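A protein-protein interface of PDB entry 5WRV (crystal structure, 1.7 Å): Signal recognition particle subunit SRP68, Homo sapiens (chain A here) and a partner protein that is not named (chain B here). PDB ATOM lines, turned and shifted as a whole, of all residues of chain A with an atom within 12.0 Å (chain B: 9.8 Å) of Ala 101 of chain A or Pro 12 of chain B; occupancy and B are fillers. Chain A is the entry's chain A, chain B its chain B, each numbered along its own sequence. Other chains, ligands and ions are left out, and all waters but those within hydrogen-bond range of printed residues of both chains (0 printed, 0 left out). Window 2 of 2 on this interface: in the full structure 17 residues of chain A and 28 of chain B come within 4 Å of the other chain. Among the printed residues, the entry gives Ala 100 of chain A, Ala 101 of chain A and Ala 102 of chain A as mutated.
OD2 of Asp 44 of chain B lies within salt-bridge range of NZ of Lys 98 of chain A, at 2.7 Å.
Among the printed residues, pairs that only touch across the chains: Leu 99 of chain A with Ser 16 of chain B, Leu 99 of chain A with Trp 15 of chain B, Lys 98 of chain A with Trp 15 of chain B, Ala 101 of chain A with Pro 12 of chain B, Leu 95 of chain A with Trp 15 of chain B and Leu 99 of chain A with Pro 12 of chain B.
Printed residues of chain B within 4 Å of Lys 98 of chain A: Trp 15 (3.6 Å) and Asp 44 (2.7 Å). Printed residues of chain B within 4 Å of Leu 99 of chain A: Pro 12 (3.95 Å), Trp 15 (3.5 Å) and Ser 16 (3.4 Å). No residue of chain B comes within 4 Å of Ala 100 of chain A. Ala 101 of chain A touches one residue of chain B. Ala 102 of chain A touches none of the printed residues of chain B. Of chain A, only Leu 99 and Ala 101 come within 4 Å of Pro 12 of chain B. No residue of chain A comes within 4 Å of Leu 14 of chain B. Of chain A, only Leu 99 (3.4 Å) comes within 4 Å of Ser 16 of chain B. The nearest residue of chain B that does not touch Ala 101 of chain A is Val 11 of chain B (6.7 Å). The nearest residue of chain A that does not touch Pro 12 of chain B is Lys 98 of chain A (4.1 Å).
Of the 9 printed residues of chain A, 4 touch a printed residue of chain B. Hydrophobic or aromatic side chains of chain A within 4 Å of the printed part of chain B: Leu 95, Leu 99 and Ala 101.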
ATOM      1  N   PRO A  94      16.922 -21.781  16.133  1.00  0.00           N
ATOM      2  CA  PRO A  94      16.900 -23.042  15.372  1.00  0.00           C
ATOM      3  C   PRO A  94      15.629 -23.185  14.532  1.00  0.00           C
ATOM      4  O   PRO A  94      14.534 -22.882  15.013  1.00  0.00           O
ATOM      5  CB  PRO A  94      16.942 -24.109  16.468  1.00  0.00           C
ATOM      6  CG  PRO A  94      17.666 -23.443  17.597  1.00  0.00           C
ATOM      7  CD  PRO A  94      17.204 -22.013  17.565  1.00  0.00           C
ATOM      8  N   LEU A  95      15.770 -23.632  13.286  1.00  0.00           N
ATOM      9  CA  LEU A  95      14.622 -23.670  12.375  1.00  0.00           C
ATOM     10  C   LEU A  95      14.136 -25.071  11.990  1.00  0.00           C
ATOM     11  O   LEU A  95      13.176 -25.200  11.221  1.00  0.00           O
ATOM     12  CB  LEU A  95      14.896 -22.841  11.112  1.00  0.00           C
ATOM     13  CG  LEU A  95      15.076 -21.324  11.289  1.00  0.00           C
ATOM     14  CD1 LEU A  95      15.201 -20.656   9.930  1.00  0.00           C
ATOM     15  CD2 LEU A  95      13.952 -20.675  12.093  1.00  0.00           C
ATOM     16  N   GLU A  96      14.775 -26.112  12.514  1.00  0.00           N
ATOM     17  CA  GLU A  96      14.476 -27.473  12.036  1.00  0.00           C
ATOM     18  C   GLU A  96      13.013 -27.882  12.266  1.00  0.00           C
ATOM     19  O   GLU A  96      12.429 -28.590  11.444  1.00  0.00           O
ATOM     20  CB  GLU A  96      15.456 -28.519  12.596  1.00  0.00           C
ATOM     21  CG  GLU A  96      15.450 -28.684  14.106  1.00  0.00           C
ATOM     22  CD  GLU A  96      16.410 -27.754  14.831  1.00  0.00           C
ATOM     23  OE1 GLU A  96      16.632 -27.986  16.035  1.00  0.00           O
ATOM     24  OE2 GLU A  96      16.944 -26.799  14.215  1.00  0.00           O
ATOM     25  N   ASP A  97      12.423 -27.416  13.364  1.00  0.00           N
ATOM     26  CA  ASP A  97      11.016 -27.723  13.658  1.00  0.00           C
ATOM     27  C   ASP A  97      10.086 -27.096  12.630  1.00  0.00           C
ATOM     28  O   ASP A  97       9.094 -27.709  12.222  1.00  0.00           O
ATOM     29  CB  ASP A  97      10.638 -27.291  15.079  1.00  0.00           C
ATOM     30  CG  ASP A  97      11.302 -28.148  16.144  1.00  0.00           C
ATOM     31  OD1 ASP A  97      11.890 -29.195  15.794  1.00  0.00           O
ATOM     32  OD2 ASP A  97      11.235 -27.780  17.334  1.00  0.00           O
ATOM     33  N   LYS A  98      10.423 -25.884  12.197  1.00  0.00           N
ATOM     34  CA  LYS A  98       9.641 -25.187  11.182  1.00  0.00           C
ATOM     35  C   LYS A  98       9.850 -25.795   9.807  1.00  0.00           C
ATOM     36  O   LYS A  98       8.905 -25.891   9.029  1.00  0.00           O
ATOM     37  CB  LYS A  98       9.961 -23.689  11.166  1.00  0.00           C
ATOM     38  CG  LYS A  98       9.537 -22.947  12.429  1.00  0.00           C
ATOM     39  CD  LYS A  98       8.017 -22.880  12.549  1.00  0.00           C
ATOM     40  CE  LYS A  98       7.604 -22.303  13.888  1.00  0.00           C
ATOM     41  NZ  LYS A  98       6.126 -22.238  14.032  1.00  0.00           N
ATOM     42  N   LEU A  99      11.082 -26.211   9.510  1.00  0.00           N
ATOM     43  CA  LEU A  99      11.364 -26.899   8.251  1.00  0.00           C
ATOM     44  C   LEU A  99      10.594 -28.216   8.140  1.00  0.00           C
ATOM     45  O   LEU A  99      10.194 -28.609   7.049  1.00  0.00           O
ATOM     46  CB  LEU A  99      12.859 -27.180   8.111  1.00  0.00           C
ATOM     47  CG  LEU A  99      13.741 -25.945   7.943  1.00  0.00           C
ATOM     48  CD1 LEU A  99      15.209 -26.345   7.986  1.00  0.00           C
ATOM     49  CD2 LEU A  99      13.425 -25.264   6.635  1.00  0.00           C
ATOM     50  N   ALA A 100      10.414 -28.884   9.275  1.00  0.00           N
ATOM     51  CA  ALA A 100       9.756 -30.191   9.338  1.00  0.00           C
ATOM     52  C   ALA A 100       8.233 -30.094   9.419  1.00  0.00           C
ATOM     53  O   ALA A 100       7.540 -31.111   9.289  1.00  0.00           O
ATOM     54  CB  ALA A 100      10.280 -30.980  10.539  1.00  0.00           C
ATOM     55  N   ALA A 101       7.730 -28.876   9.629  1.00  0.00           N
ATOM     56  CA  ALA A 101       6.305 -28.602   9.889  1.00  0.00           C
ATOM     57  C   ALA A 101       5.814 -29.318  11.149  1.00  0.00           C
ATOM     58  O   ALA A 101       4.715 -29.884  11.176  1.00  0.00           O
ATOM     59  CB  ALA A 101       5.433 -28.936   8.668  1.00  0.00           C
ATOM     60  N   ALA A 102       6.645 -29.276  12.190  1.00  0.00           N
ATOM     61  CA  ALA A 102       6.365 -29.944  13.461  1.00  0.00           C
ATOM     62  C   ALA A 102       5.300 -29.211  14.273  1.00  0.00           C
ATOM     63  O   ALA A 102       5.309 -27.983  14.364  1.00  0.00           O
ATOM     64  CB  ALA A 102       7.651 -30.083  14.280  1.00  0.00           C
ATOM     65  N   VAL B   9       5.931 -21.848  -1.709  1.00  0.00           N
ATOM     66  CA  VAL B   9       4.448 -21.954  -1.863  1.00  0.00           C
ATOM     67  C   VAL B   9       3.786 -22.417  -0.564  1.00  0.00           C
ATOM     68  O   VAL B   9       2.996 -21.679   0.026  1.00  0.00           O
ATOM     69  CB  VAL B   9       4.058 -22.883  -3.032  1.00  0.00           C
ATOM     70  N   SER B  10       4.110 -23.634  -0.120  1.00  0.00           N
ATOM     71  CA  SER B  10       3.685 -24.116   1.195  1.00  0.00           C
ATOM     72  C   SER B  10       4.504 -23.407   2.275  1.00  0.00           C
ATOM     73  O   SER B  10       5.585 -22.873   1.987  1.00  0.00           O
ATOM     74  CB  SER B  10       3.868 -25.635   1.311  1.00  0.00           C
ATOM     75  OG  SER B  10       5.231 -25.982   1.519  1.00  0.00           O
ATOM     76  N   VAL B  11       3.994 -23.408   3.504  1.00  0.00           N
ATOM     77  CA  VAL B  11       4.688 -22.783   4.638  1.00  0.00           C
ATOM     78  C   VAL B  11       6.063 -23.424   4.918  1.00  0.00           C
ATOM     79  O   VAL B  11       7.051 -22.694   5.053  1.00  0.00           O
ATOM     80  CB  VAL B  11       3.801 -22.718   5.904  1.00  0.00           C
ATOM     81  CG1 VAL B  11       4.601 -22.253   7.111  1.00  0.00           C
ATOM     82  CG2 VAL B  11       2.620 -21.784   5.667  1.00  0.00           C
ATOM     83  N   PRO B  12       6.144 -24.773   4.979  1.00  0.00           N
ATOM     84  CA  PRO B  12       7.472 -25.398   5.174  1.00  0.00           C
ATOM     85  C   PRO B  12       8.480 -25.070   4.071  1.00  0.00           C
ATOM     86  O   PRO B  12       9.685 -24.970   4.348  1.00  0.00           O
ATOM     87  CB  PRO B  12       7.164 -26.899   5.172  1.00  0.00           C
ATOM     88  CG  PRO B  12       5.723 -26.996   5.552  1.00  0.00           C
ATOM     89  CD  PRO B  12       5.063 -25.783   4.972  1.00  0.00           C
ATOM     90  N   ALA B  13       7.999 -24.918   2.836  1.00  0.00           N
ATOM     91  CA  ALA B  13       8.844 -24.504   1.723  1.00  0.00           C
ATOM     92  C   ALA B  13       9.313 -23.056   1.892  1.00  0.00           C
ATOM     93  O   ALA B  13      10.445 -22.724   1.543  1.00  0.00           O
ATOM     94  CB  ALA B  13       8.118 -24.678   0.396  1.00  0.00           C
ATOM     95  N   LEU B  14       8.444 -22.197   2.419  1.00  0.00           N
ATOM     96  CA  LEU B  14       8.836 -20.822   2.733  1.00  0.00           C
ATOM     97  C   LEU B  14       9.931 -20.824   3.800  1.00  0.00           C
ATOM     98  O   LEU B  14      10.914 -20.090   3.695  1.00  0.00           O
ATOM     99  CB  LEU B  14       7.630 -19.995   3.193  1.00  0.00           C
ATOM    100  CG  LEU B  14       6.589 -19.646   2.121  1.00  0.00           C
ATOM    101  CD1 LEU B  14       5.357 -19.017   2.756  1.00  0.00           C
ATOM    102  CD2 LEU B  14       7.166 -18.726   1.054  1.00  0.00           C
ATOM    103  N   TRP B  15       9.766 -21.661   4.818  1.00  0.00           N
ATOM    104  CA  TRP B  15      10.787 -21.796   5.872  1.00  0.00           C
ATOM    105  C   TRP B  15      12.109 -22.265   5.333  1.00  0.00           C
ATOM    106  O   TRP B  15      13.175 -21.828   5.801  1.00  0.00           O
ATOM    107  CB  TRP B  15      10.303 -22.718   6.974  1.00  0.00           C
ATOM    108  CG  TRP B  15       9.422 -22.005   7.965  1.00  0.00           C
ATOM    109  CD1 TRP B  15       8.059 -22.200   8.194  1.00  0.00           C
ATOM    110  CD2 TRP B  15       9.824 -20.943   8.891  1.00  0.00           C
ATOM    111  NE1 TRP B  15       7.607 -21.354   9.176  1.00  0.00           N
ATOM    112  CE2 TRP B  15       8.618 -20.568   9.635  1.00  0.00           C
ATOM    113  CE3 TRP B  15      11.026 -20.284   9.165  1.00  0.00           C
ATOM    114  CZ2 TRP B  15       8.634 -19.579  10.614  1.00  0.00           C
ATOM    115  CZ3 TRP B  15      11.029 -19.287  10.149  1.00  0.00           C
ATOM    116  CH2 TRP B  15       9.861 -18.943  10.856  1.00  0.00           C
ATOM    117  N   SER B  16      12.059 -23.149   4.334  1.00  0.00           N
ATOM    118  CA  SER B  16      13.281 -23.596   3.656  1.00  0.00           C
ATOM    119  C   SER B  16      14.032 -22.410   3.038  1.00  0.00           C
ATOM    120  O   SER B  16      15.266 -22.338   3.113  1.00  0.00           O
ATOM    121  CB  SER B  16      12.956 -24.654   2.592  1.00  0.00           C
ATOM    122  OG  SER B  16      14.144 -25.086   1.945  1.00  0.00           O
ATOM    123  N   GLU B  17      13.281 -21.483   2.442  1.00  0.00           N
ATOM    124  CA  GLU B  17      13.853 -20.281   1.848  1.00  0.00           C
ATOM    125  C   GLU B  17      14.382 -19.337   2.929  1.00  0.00           C
ATOM    126  O   GLU B  17      15.466 -18.768   2.768  1.00  0.00           O
ATOM    127  CB  GLU B  17      12.829 -19.552   0.972  1.00  0.00           C
ATOM    128  CG  GLU B  17      12.548 -20.221  -0.368  1.00  0.00           C
ATOM    129  CD  GLU B  17      11.714 -19.341  -1.277  1.00  0.00           C
ATOM    130  OE1 GLU B  17      10.557 -19.045  -0.917  1.00  0.00           O
ATOM    131  OE2 GLU B  17      12.216 -18.941  -2.350  1.00  0.00           O
ATOM    132  N   VAL B  18      13.625 -19.173   4.020  1.00  0.00           N
ATOM    133  CA  VAL B  18      14.097 -18.359   5.158  1.00  0.00           C
ATOM    134  C   VAL B  18      15.470 -18.856   5.615  1.00  0.00           C
ATOM    135  O   VAL B  18      16.420 -18.066   5.750  1.00  0.00           O
ATOM    136  CB  VAL B  18      13.101 -18.345   6.346  1.00  0.00           C
ATOM    137  CG1 VAL B  18      13.720 -17.678   7.579  1.00  0.00           C
ATOM    138  CG2 VAL B  18      11.816 -17.624   5.952  1.00  0.00           C
ATOM    139  N   ASN B  19      15.579 -20.165   5.831  1.00  0.00           N
ATOM    140  CA  ASN B  19      16.846 -20.746   6.268  1.00  0.00           C
ATOM    141  C   ASN B  19      17.966 -20.507   5.261  1.00  0.00           C
ATOM    142  O   ASN B  19      19.064 -20.095   5.657  1.00  0.00           O
ATOM    143  CB  ASN B  19      16.709 -22.239   6.568  1.00  0.00           C
ATOM    144  CG  ASN B  19      18.018 -22.855   7.025  1.00  0.00           C
ATOM    145  OD1 ASN B  19      18.431 -22.676   8.171  1.00  0.00           O
ATOM    146  ND2 ASN B  19      18.684 -23.576   6.124  1.00  0.00           N
ATOM    147  N   ARG B  20      17.692 -20.751   3.973  1.00  0.00           N
ATOM    148  CA  ARG B  20      18.721 -20.589   2.942  1.00  0.00           C
ATOM    149  C   ARG B  20      19.219 -19.143   2.878  1.00  0.00           C
ATOM    150  O   ARG B  20      20.438 -18.898   2.849  1.00  0.00           O
ATOM    151  CB  ARG B  20      18.229 -21.053   1.565  1.00  0.00           C
ATOM    152  CG  ARG B  20      19.309 -20.961   0.488  1.00  0.00           C
ATOM    153  CD  ARG B  20      18.879 -21.571  -0.836  1.00  0.00           C
ATOM    154  NE  ARG B  20      17.774 -20.850  -1.475  1.00  0.00           N
ATOM    155  CZ  ARG B  20      17.898 -19.740  -2.203  1.00  0.00           C
ATOM    156  NH1 ARG B  20      19.085 -19.173  -2.392  1.00  0.00           N
ATOM    157  NH2 ARG B  20      16.819 -19.188  -2.741  1.00  0.00           N
ATOM    158  N   THR B  33      10.461 -13.184   2.697  1.00  0.00           N
ATOM    159  CA  THR B  33       9.899 -14.522   2.882  1.00  0.00           C
ATOM    160  C   THR B  33       9.200 -14.668   4.238  1.00  0.00           C
ATOM    161  O   THR B  33       8.094 -15.220   4.318  1.00  0.00           O
ATOM    162  CB  THR B  33      10.989 -15.610   2.715  1.00  0.00           C
ATOM    163  OG1 THR B  33      11.728 -15.358   1.514  1.00  0.00           O
ATOM    164  CG2 THR B  33      10.368 -17.001   2.636  1.00  0.00           C
ATOM    165  N   ILE B  37       5.225 -15.627   5.471  1.00  0.00           N
ATOM    166  CA  ILE B  37       4.840 -16.584   6.516  1.00  0.00           C
ATOM    167  C   ILE B  37       3.918 -15.927   7.550  1.00  0.00           C
ATOM    168  O   ILE B  37       2.945 -16.539   8.005  1.00  0.00           O
ATOM    169  CB  ILE B  37       6.073 -17.216   7.208  1.00  0.00           C
ATOM    170  CG1 ILE B  37       6.862 -18.067   6.203  1.00  0.00           C
ATOM    171  CG2 ILE B  37       5.660 -18.060   8.411  1.00  0.00           C
ATOM    172  CD1 ILE B  37       8.215 -18.553   6.702  1.00  0.00           C
ATOM    173  N   ILE B  40       0.302 -15.626   6.702  1.00  0.00           N
ATOM    174  CA  ILE B  40      -0.406 -16.897   6.880  1.00  0.00           C
ATOM    175  C   ILE B  40      -0.586 -17.240   8.362  1.00  0.00           C
ATOM    176  O   ILE B  40      -1.682 -17.622   8.789  1.00  0.00           O
ATOM    177  CB  ILE B  40       0.315 -18.037   6.121  1.00  0.00           C
ATOM    178  CG1 ILE B  40       0.375 -17.711   4.621  1.00  0.00           C
ATOM    179  CG2 ILE B  40      -0.367 -19.381   6.363  1.00  0.00           C
ATOM    180  CD1 ILE B  40       1.368 -18.529   3.821  1.00  0.00           C
ATOM    181  N   ASN B  41       0.484 -17.095   9.141  1.00  0.00           N
ATOM    182  CA  ASN B  41       0.461 -17.362  10.577  1.00  0.00           C
ATOM    183  C   ASN B  41       0.888 -16.108  11.349  1.00  0.00           C
ATOM    184  O   ASN B  41       2.062 -15.952  11.686  1.00  0.00           O
ATOM    185  CB  ASN B  41       1.374 -18.555  10.919  1.00  0.00           C
ATOM    186  CG  ASN B  41       0.986 -19.835  10.182  1.00  0.00           C
ATOM    187  OD1 ASN B  41       1.844 -20.540   9.643  1.00  0.00           O
ATOM    188  ND2 ASN B  41      -0.304 -20.146  10.161  1.00  0.00           N
ATOM    189  N   ASP B  44       3.128 -16.235  14.677  1.00  0.00           N
ATOM    190  CA  ASP B  44       4.156 -17.269  14.729  1.00  0.00           C
ATOM    191  C   ASP B  44       5.394 -16.669  15.394  1.00  0.00           C
ATOM    192  O   ASP B  44       5.984 -15.725  14.876  1.00  0.00           O
ATOM    193  CB  ASP B  44       4.475 -17.780  13.317  1.00  0.00           C
ATOM    194  CG  ASP B  44       5.400 -18.983  13.321  1.00  0.00           C
ATOM    195  OD1 ASP B  44       6.587 -18.824  13.662  1.00  0.00           O
ATOM    196  OD2 ASP B  44       4.946 -20.095  12.971  1.00  0.00           O
